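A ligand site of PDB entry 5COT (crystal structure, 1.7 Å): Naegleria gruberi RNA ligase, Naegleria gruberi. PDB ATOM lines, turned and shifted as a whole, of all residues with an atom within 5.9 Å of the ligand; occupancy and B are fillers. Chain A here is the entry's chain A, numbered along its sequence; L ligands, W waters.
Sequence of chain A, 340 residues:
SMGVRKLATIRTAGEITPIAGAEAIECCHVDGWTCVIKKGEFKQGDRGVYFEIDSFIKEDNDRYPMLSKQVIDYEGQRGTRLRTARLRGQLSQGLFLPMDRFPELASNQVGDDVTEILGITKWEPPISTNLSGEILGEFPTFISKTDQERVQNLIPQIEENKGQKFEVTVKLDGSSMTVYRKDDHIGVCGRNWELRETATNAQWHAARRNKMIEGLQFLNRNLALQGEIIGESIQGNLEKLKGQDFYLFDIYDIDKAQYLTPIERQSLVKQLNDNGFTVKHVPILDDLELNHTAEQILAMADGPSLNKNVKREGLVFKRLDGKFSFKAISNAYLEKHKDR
An oxygen (O5) of the ligand lies within hydrogen-bond range of the backbone carbonyl oxygen (O) of Thr 146, at 3.1 Å. The side-chain amino group of Lys 171 is covalently linked to a phosphorus (P1) of the ligand, 1.8 Å away. NZ of Lys 327 lies within salt-bridge range of O2 of the ligand (2.9 Å). The side-chain hydroxyl (OG1) of Thr 169 lies within hydrogen-bond range of a nitrogen (N3) of the ligand (2.9 Å). OG1 of Thr 146 sits at hydrogen-bond distance from O5 of the ligand (2.7 Å). N4 of the ligand lies within hydrogen-bond range of NZ of Lys 318. O6 of the ligand lies within hydrogen-bond range of OE1 of Glu 228 (2.6 Å). A nitrogen (N2) of the ligand is in hydrogen-bond range of the backbone NH (N) of Leu 172, 3.0 Å away. N3 of the ligand lies within hydrogen-bond range of O of Val 170 (2.8 Å).
NZ of Lys 318 lies within hydrogen-bond range of OG1 of Thr 169, 3.2 Å away. NZ of Lys 171 is in salt-bridge range of OE1 of Glu 313 (3.8 Å). OG1 of Thr 146 sits at hydrogen-bond distance from OG of Ser 176 (2.8 Å). The side-chain carboxylate of Glu 228 sits at hydrogen-bond distance from the backbone NH of Ser 175, at 3.2 Å. O of Ser 176 is in hydrogen-bond range of N of Arg 191 (3.2 Å). N of Val 170 is in hydrogen-bond range of O of Pro 283 (2.9 Å). The backbone carbonyl oxygen (O) of Thr 169 is in hydrogen-bond range of the backbone NH (N) of Val 316 (2.9 Å).
Ser 176 touches the ligand (CB to O6, 3.3 Å). Phe 249 touches the ligand (CD2 to C10, 3.4 Å). Val 282 touches the ligand. Val 316 touches the ligand. CD1 of Ile 329 touches O2 of the ligand, at 3.7 Å. Hydrophobic or aromatic side chains within 4 Å of the ligand: Phe 249, Val 282, Val 316 and Ile 329.
Water W3 lies within hydrogen-bond range of O of Thr 146, N5 of the ligand and NE2 of Gln 148. Water W4 lies within hydrogen-bond range of the side-chain amino group (NZ) of Lys 327 (2.8 Å), the backbone NH (N) of Gln 148 (3.0 Å) and an oxygen (O3) of the ligand (3.2 Å).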
ATOM      1  N   THR A 146       9.719 -14.183   9.976  1.00  0.00           N
ATOM      2  CA  THR A 146      10.437 -13.930  11.227  1.00  0.00           C
ATOM      3  C   THR A 146      11.466 -14.993  11.649  1.00  0.00           C
ATOM      4  O   THR A 146      11.961 -14.970  12.780  1.00  0.00           O
ATOM      5  CB  THR A 146       9.405 -13.689  12.364  1.00  0.00           C
ATOM      6  OG1 THR A 146       8.643 -14.865  12.603  1.00  0.00           O
ATOM      7  CG2 THR A 146       8.452 -12.558  11.996  1.00  0.00           C
ATOM      8  N   ASP A 147      11.808 -15.912  10.781  1.00  0.00           N
ATOM      9  CA  ASP A 147      12.757 -17.013  11.146  1.00  0.00           C
ATOM     10  C   ASP A 147      14.103 -16.411  11.477  1.00  0.00           C
ATOM     11  O   ASP A 147      14.472 -15.348  10.983  1.00  0.00           O
ATOM     12  CB  ASP A 147      12.856 -17.972   9.915  1.00  0.00           C
ATOM     13  CG  ASP A 147      11.502 -18.579   9.619  1.00  0.00           C
ATOM     14  OD1 ASP A 147      11.047 -19.385  10.392  1.00  0.00           O
ATOM     15  OD2 ASP A 147      10.776 -18.131   8.713  1.00  0.00           O
ATOM     16  N   GLN A 148      14.843 -17.052  12.390  1.00  0.00           N
ATOM     17  CA  GLN A 148      16.135 -16.588  12.799  1.00  0.00           C
ATOM     18  C   GLN A 148      17.098 -17.782  12.700  1.00  0.00           C
ATOM     19  O   GLN A 148      16.774 -18.897  13.115  1.00  0.00           O
ATOM     20  CB  GLN A 148      16.109 -16.171  14.264  1.00  0.00           C
ATOM     21  CG  GLN A 148      15.283 -14.933  14.530  1.00  0.00           C
ATOM     22  CD  GLN A 148      15.884 -13.689  13.960  1.00  0.00           C
ATOM     23  OE1 GLN A 148      17.021 -13.669  13.433  1.00  0.00           O
ATOM     24  NE2 GLN A 148      15.069 -12.659  13.902  1.00  0.00           N
ATOM     25  N   ARG A 150      20.329 -19.984  13.810  1.00  0.00           N
ATOM     26  CA  ARG A 150      21.014 -20.366  15.052  1.00  0.00           C
ATOM     27  C   ARG A 150      22.465 -19.970  15.137  1.00  0.00           C
ATOM     28  O   ARG A 150      23.220 -20.114  14.159  1.00  0.00           O
ATOM     29  CB  ARG A 150      20.986 -21.879  15.201  1.00  0.00           C
ATOM     30  CG  ARG A 150      19.628 -22.474  15.520  1.00  0.00           C
ATOM     31  CD  ARG A 150      19.725 -23.948  15.698  1.00  0.00           C
ATOM     32  NE  ARG A 150      18.537 -24.548  16.281  1.00  0.00           N
ATOM     33  CZ  ARG A 150      17.597 -25.120  15.575  1.00  0.00           C
ATOM     34  NH1 ARG A 150      17.729 -25.246  14.260  1.00  0.00           N
ATOM     35  NH2 ARG A 150      16.531 -25.630  16.212  1.00  0.00           N
ATOM     36  N   THR A 169      17.106  -9.837  23.366  1.00  0.00           N
ATOM     37  CA  THR A 169      15.769  -9.997  23.873  1.00  0.00           C
ATOM     38  C   THR A 169      15.494 -11.420  24.246  1.00  0.00           C
ATOM     39  O   THR A 169      16.109 -12.403  23.726  1.00  0.00           O
ATOM     40  CB  THR A 169      14.712  -9.534  22.885  1.00  0.00           C
ATOM     41  OG1 THR A 169      14.973 -10.146  21.604  1.00  0.00           O
ATOM     42  CG2 THR A 169      14.650  -7.988  22.732  1.00  0.00           C
ATOM     43  N   VAL A 170      14.574 -11.566  25.217  1.00  0.00           N
ATOM     44  CA  VAL A 170      14.093 -12.902  25.549  1.00  0.00           C
ATOM     45  C   VAL A 170      13.249 -13.506  24.429  1.00  0.00           C
ATOM     46  O   VAL A 170      12.342 -12.859  23.868  1.00  0.00           O
ATOM     47  CB  VAL A 170      13.325 -12.905  26.869  1.00  0.00           C
ATOM     48  CG1 VAL A 170      12.745 -14.271  27.152  1.00  0.00           C
ATOM     49  CG2 VAL A 170      14.247 -12.461  28.003  1.00  0.00           C
ATOM     50  N   LYS A 171      13.589 -14.752  24.080  1.00  0.00           N
ATOM     51  CA  LYS A 171      12.818 -15.497  23.060  1.00  0.00           C
ATOM     52  C   LYS A 171      11.622 -16.142  23.748  1.00  0.00           C
ATOM     53  O   LYS A 171      11.780 -16.978  24.651  1.00  0.00           O
ATOM     54  CB  LYS A 171      13.652 -16.605  22.430  1.00  0.00           C
ATOM     55  CG  LYS A 171      13.087 -17.226  21.147  1.00  0.00           C
ATOM     56  CD  LYS A 171      14.048 -18.289  20.672  1.00  0.00           C
ATOM     57  CE  LYS A 171      13.932 -18.598  19.225  1.00  0.00           C
ATOM     58  NZ  LYS A 171      12.628 -19.147  18.855  1.00  0.00           N
ATOM     59  N   LEU A 172      10.416 -15.721  23.363  1.00  0.00           N
ATOM     60  CA  LEU A 172       9.164 -16.256  23.912  1.00  0.00           C
ATOM     61  C   LEU A 172       8.651 -17.384  23.087  1.00  0.00           C
ATOM     62  O   LEU A 172       8.728 -17.358  21.850  1.00  0.00           O
ATOM     63  CB  LEU A 172       8.114 -15.145  24.021  1.00  0.00           C
ATOM     64  CG  LEU A 172       8.488 -13.960  24.839  1.00  0.00           C
ATOM     65  CD1 LEU A 172       7.403 -12.899  24.705  1.00  0.00           C
ATOM     66  CD2 LEU A 172       8.891 -14.313  26.264  1.00  0.00           C
ATOM     67  N   ASP A 173       8.086 -18.387  23.778  1.00  0.00           N
ATOM     68  CA  ASP A 173       7.625 -19.578  23.125  1.00  0.00           C
ATOM     69  C   ASP A 173       6.148 -19.496  22.818  1.00  0.00           C
ATOM     70  O   ASP A 173       5.300 -19.937  23.619  1.00  0.00           O
ATOM     71  CB  ASP A 173       8.056 -20.812  23.913  1.00  0.00           C
ATOM     72  CG  ASP A 173       7.877 -22.100  23.163  1.00  0.00           C
ATOM     73  OD1 ASP A 173       7.329 -22.227  22.048  1.00  0.00           O
ATOM     74  OD2 ASP A 173       8.345 -23.114  23.772  1.00  0.00           O
ATOM     75  N   SER A 175       3.644 -18.188  19.066  1.00  0.00           N
ATOM     76  CA  SER A 175       3.488 -18.288  17.625  1.00  0.00           C
ATOM     77  C   SER A 175       3.761 -16.901  17.028  1.00  0.00           C
ATOM     78  O   SER A 175       3.436 -15.899  17.620  1.00  0.00           O
ATOM     79  CB  SER A 175       2.108 -18.782  17.314  1.00  0.00           C
ATOM     80  OG  SER A 175       1.934 -18.943  15.929  1.00  0.00           O
ATOM     81  N   SER A 176       4.398 -16.846  15.869  1.00  0.00           N
ATOM     82  CA  SER A 176       4.724 -15.571  15.237  1.00  0.00           C
ATOM     83  C   SER A 176       3.458 -14.976  14.649  1.00  0.00           C
ATOM     84  O   SER A 176       2.646 -15.678  13.973  1.00  0.00           O
ATOM     85  CB  SER A 176       5.656 -15.836  14.043  1.00  0.00           C
ATOM     86  OG  SER A 176       5.998 -14.608  13.448  1.00  0.00           O
ATOM     87  N   MET A 177       3.313 -13.690  14.847  1.00  0.00           N
ATOM     88  CA  MET A 177       2.149 -12.931  14.392  1.00  0.00           C
ATOM     89  C   MET A 177       2.567 -11.637  13.777  1.00  0.00           C
ATOM     90  O   MET A 177       3.444 -11.002  14.299  1.00  0.00           O
ATOM     91  CB  MET A 177       1.269 -12.695  15.660  1.00  0.00           C
ATOM     92  CG  MET A 177       0.139 -11.722  15.491  1.00  0.00           C
ATOM     93  SD  MET A 177      -0.893 -11.792  16.961  1.00  0.00           S
ATOM     94  CE  MET A 177      -1.694 -10.214  16.616  1.00  0.00           C
ATOM     95  N   ARG A 191       2.013 -17.177  11.199  1.00  0.00           N
ATOM     96  CA  ARG A 191       3.321 -17.397  10.693  1.00  0.00           C
ATOM     97  C   ARG A 191       3.450 -17.461   9.164  1.00  0.00           C
ATOM     98  O   ARG A 191       4.417 -16.957   8.582  1.00  0.00           O
ATOM     99  CB  ARG A 191       3.836 -18.736  11.336  1.00  0.00           C
ATOM    100  CG  ARG A 191       5.230 -19.058  10.971  1.00  0.00           C
ATOM    101  CD  ARG A 191       5.544 -20.438  11.492  1.00  0.00           C
ATOM    102  NE  ARG A 191       6.913 -20.786  11.210  1.00  0.00           N
ATOM    103  CZ  ARG A 191       7.419 -21.975  11.542  1.00  0.00           C
ATOM    104  NH1 ARG A 191       6.630 -22.895  12.104  1.00  0.00           N
ATOM    105  NH2 ARG A 191       8.691 -22.247  11.274  1.00  0.00           N
ATOM    106  N   GLY A 227       5.549  -9.916  16.079  1.00  0.00           N
ATOM    107  CA  GLY A 227       5.748 -10.287  17.462  1.00  0.00           C
ATOM    108  C   GLY A 227       5.292 -11.666  17.760  1.00  0.00           C
ATOM    109  O   GLY A 227       4.911 -12.369  16.833  1.00  0.00           O
ATOM    110  N   GLU A 228       5.352 -12.045  19.026  1.00  0.00           N
ATOM    111  CA  GLU A 228       4.977 -13.370  19.456  1.00  0.00           C
ATOM    112  C   GLU A 228       3.639 -13.208  20.157  1.00  0.00           C
ATOM    113  O   GLU A 228       3.539 -12.437  21.142  1.00  0.00           O
ATOM    114  CB  GLU A 228       6.013 -14.028  20.379  1.00  0.00           C
ATOM    115  CG  GLU A 228       5.973 -15.522  20.493  1.00  0.00           C
ATOM    116  CD  GLU A 228       6.577 -16.225  19.286  1.00  0.00           C
ATOM    117  OE1 GLU A 228       6.876 -15.514  18.274  1.00  0.00           O
ATOM    118  OE2 GLU A 228       6.712 -17.455  19.314  1.00  0.00           O
ATOM    119  N   PHE A 249       8.557  -7.829  18.680  1.00  0.00           N
ATOM    120  CA  PHE A 249       9.995  -7.979  18.608  1.00  0.00           C
ATOM    121  C   PHE A 249      10.622  -7.302  17.392  1.00  0.00           C
ATOM    122  O   PHE A 249      11.851  -7.143  17.402  1.00  0.00           O
ATOM    123  CB  PHE A 249      10.446  -9.466  18.755  1.00  0.00           C
ATOM    124  CG  PHE A 249       9.787 -10.422  17.771  1.00  0.00           C
ATOM    125  CD1 PHE A 249       9.999 -10.320  16.390  1.00  0.00           C
ATOM    126  CD2 PHE A 249       8.946 -11.471  18.245  1.00  0.00           C
ATOM    127  CE1 PHE A 249       9.423 -11.232  15.516  1.00  0.00           C
ATOM    128  CE2 PHE A 249       8.334 -12.320  17.370  1.00  0.00           C
ATOM    129  CZ  PHE A 249       8.550 -12.218  16.014  1.00  0.00           C
ATOM    130  N   ASP A 250       9.825  -7.004  16.347  1.00  0.00           N
ATOM    131  CA  ASP A 250      10.382  -6.336  15.144  1.00  0.00           C
ATOM    132  C   ASP A 250       9.298  -5.519  14.414  1.00  0.00           C
ATOM    133  O   ASP A 250       8.093  -5.791  14.568  1.00  0.00           O
ATOM    134  CB  ASP A 250      10.928  -7.373  14.197  1.00  0.00           C
ATOM    135  CG  ASP A 250      12.425  -7.576  14.292  1.00  0.00           C
ATOM    136  OD1 ASP A 250      13.220  -6.552  14.298  1.00  0.00           O
ATOM    137  OD2 ASP A 250      12.833  -8.785  14.296  1.00  0.00           O
ATOM    138  N   VAL A 282       8.588  -7.839  23.676  1.00  0.00           N
ATOM    139  CA  VAL A 282       9.391  -8.856  24.301  1.00  0.00           C
ATOM    140  C   VAL A 282      10.406  -8.267  25.296  1.00  0.00           C
ATOM    141  O   VAL A 282      10.838  -7.098  25.120  1.00  0.00           O
ATOM    142  CB  VAL A 282      10.144  -9.756  23.248  1.00  0.00           C
ATOM    143  CG1 VAL A 282       9.181 -10.495  22.362  1.00  0.00           C
ATOM    144  CG2 VAL A 282      11.130  -8.936  22.446  1.00  0.00           C
ATOM    145  N   PRO A 283      10.712  -8.984  26.381  1.00  0.00           N
ATOM    146  CA  PRO A 283      11.685  -8.467  27.304  1.00  0.00           C
ATOM    147  C   PRO A 283      13.063  -8.139  26.668  1.00  0.00           C
ATOM    148  O   PRO A 283      13.588  -8.952  25.859  1.00  0.00           O
ATOM    149  CB  PRO A 283      11.869  -9.607  28.308  1.00  0.00           C
ATOM    150  CG  PRO A 283      10.571 -10.281  28.291  1.00  0.00           C
ATOM    151  CD  PRO A 283      10.172 -10.260  26.824  1.00  0.00           C
ATOM    152  N   GLU A 313      13.137 -19.945  26.859  1.00  0.00           N
ATOM    153  CA  GLU A 313      13.494 -20.695  25.679  1.00  0.00           C
ATOM    154  C   GLU A 313      14.870 -20.360  25.184  1.00  0.00           C
ATOM    155  O   GLU A 313      15.562 -21.218  24.648  1.00  0.00           O
ATOM    156  CB  GLU A 313      12.453 -20.457  24.603  1.00  0.00           C
ATOM    157  CG  GLU A 313      12.701 -21.346  23.346  1.00  0.00           C
ATOM    158  CD  GLU A 313      11.658 -21.153  22.249  1.00  0.00           C
ATOM    159  OE1 GLU A 313      10.974 -20.092  22.176  1.00  0.00           O
ATOM    160  OE2 GLU A 313      11.602 -22.067  21.410  1.00  0.00           O
ATOM    161  N   VAL A 316      17.253 -13.824  21.531  1.00  0.00           N
ATOM    162  CA  VAL A 316      17.462 -13.361  20.139  1.00  0.00           C
ATOM    163  C   VAL A 316      18.337 -12.119  20.208  1.00  0.00           C
ATOM    164  O   VAL A 316      18.174 -11.250  21.060  1.00  0.00           O
ATOM    165  CB  VAL A 316      16.121 -13.136  19.415  1.00  0.00           C
ATOM    166  CG1 VAL A 316      16.381 -12.622  18.031  1.00  0.00           C
ATOM    167  CG2 VAL A 316      15.296 -14.383  19.424  1.00  0.00           C
ATOM    168  N   LYS A 318      19.835  -8.978  17.953  1.00  0.00           N
ATOM    169  CA  LYS A 318      19.581  -8.157  16.813  1.00  0.00           C
ATOM    170  C   LYS A 318      20.579  -7.035  16.759  1.00  0.00           C
ATOM    171  O   LYS A 318      20.625  -6.149  17.640  1.00  0.00           O
ATOM    172  CB  LYS A 318      18.131  -7.600  16.709  1.00  0.00           C
ATOM    173  CG  LYS A 318      17.084  -8.692  16.789  1.00  0.00           C
ATOM    174  CD  LYS A 318      15.678  -8.110  16.835  1.00  0.00           C
ATOM    175  CE  LYS A 318      14.681  -9.248  16.988  1.00  0.00           C
ATOM    176  NZ  LYS A 318      14.568  -9.594  18.431  1.00  0.00           N
ATOM    177  N   LYS A 327      19.419 -16.387  16.760  1.00  0.00           N
ATOM    178  CA  LYS A 327      18.848 -16.902  18.026  1.00  0.00           C
ATOM    179  C   LYS A 327      19.877 -17.834  18.727  1.00  0.00           C
ATOM    180  O   LYS A 327      20.680 -18.485  18.107  1.00  0.00           O
ATOM    181  CB  LYS A 327      17.561 -17.661  17.762  1.00  0.00           C
ATOM    182  CG  LYS A 327      17.684 -18.933  16.946  1.00  0.00           C
ATOM    183  CD  LYS A 327      16.288 -19.466  16.571  1.00  0.00           C
ATOM    184  CE  LYS A 327      16.323 -20.658  15.659  1.00  0.00           C
ATOM    185  NZ  LYS A 327      15.016 -21.145  15.149  1.00  0.00           N
ATOM    186  N   ILE A 329      19.181 -20.705  21.398  1.00  0.00           N
ATOM    187  CA  ILE A 329      18.193 -21.478  22.159  1.00  0.00           C
ATOM    188  C   ILE A 329      18.900 -22.130  23.340  1.00  0.00           C
ATOM    189  O   ILE A 329      19.963 -22.709  23.155  1.00  0.00           O
ATOM    190  CB  ILE A 329      17.487 -22.485  21.228  1.00  0.00           C
ATOM    191  CG1 ILE A 329      16.653 -21.747  20.171  1.00  0.00           C
ATOM    192  CG2 ILE A 329      16.611 -23.469  21.988  1.00  0.00           C
ATOM    193  CD1 ILE A 329      16.303 -22.572  18.967  1.00  0.00           C
HETATM  194  P1  LIG L   1      12.281 -20.033  17.385  1.00  0.00           P
HETATM  195  O1  LIG L   1      10.776 -20.301  17.236  1.00  0.00           O
HETATM  196  O2  LIG L   1      13.239 -21.208  17.411  1.00  0.00           O
HETATM  197  O3  LIG L   1      12.867 -19.072  16.155  1.00  0.00           O
HETATM  198  C1  LIG L   1      12.434 -17.782  15.716  1.00  0.00           C
HETATM  199  C2  LIG L   1      11.034 -17.423  16.182  1.00  0.00           C
HETATM  200  O4  LIG L   1      11.070 -16.932  17.546  1.00  0.00           O
HETATM  201  C3  LIG L   1      10.504 -16.253  15.369  1.00  0.00           C
HETATM  202  O5  LIG L   1       9.870 -16.713  14.196  1.00  0.00           O
HETATM  203  C4  LIG L   1       9.497 -15.645  16.324  1.00  0.00           C
HETATM  204  O6  LIG L   1       8.161 -16.171  16.158  1.00  0.00           O
HETATM  205  C5  LIG L   1       9.926 -16.018  17.744  1.00  0.00           C
HETATM  206  N1  LIG L   1      10.327 -15.027  18.679  1.00  0.00           N
HETATM  207  C6  LIG L   1      10.040 -15.080  20.015  1.00  0.00           C
HETATM  208  N2  LIG L   1      10.639 -14.219  20.727  1.00  0.00           N
HETATM  209  C7  LIG L   1      11.438 -13.501  19.833  1.00  0.00           C
HETATM  210  C8  LIG L   1      12.359 -12.397  20.009  1.00  0.00           C
HETATM  211  N3  LIG L   1      12.677 -11.906  21.210  1.00  0.00           N
HETATM  212  N4  LIG L   1      12.947 -11.947  18.881  1.00  0.00           N
HETATM  213  C9  LIG L   1      12.582 -12.456  17.671  1.00  0.00           C
HETATM  214  N5  LIG L   1      11.806 -13.531  17.441  1.00  0.00           N
HETATM  215  C10 LIG L   1      11.173 -14.040  18.518  1.00  0.00           C
HETATM  216  O   HOH W   1       8.111 -18.643  14.048  1.00  0.00           O
HETATM  217  O   HOH W   2      12.174 -23.487  15.883  1.00  0.00           O
HETATM  218  O   HOH W   3      12.246 -13.091  14.576  1.00  0.00           O
HETATM  219  O   HOH W   4      13.652 -19.715  13.108  1.00  0.00           O
HETATM  220  O   HOH W   5       9.955 -20.601  14.725  1.00  0.00           O
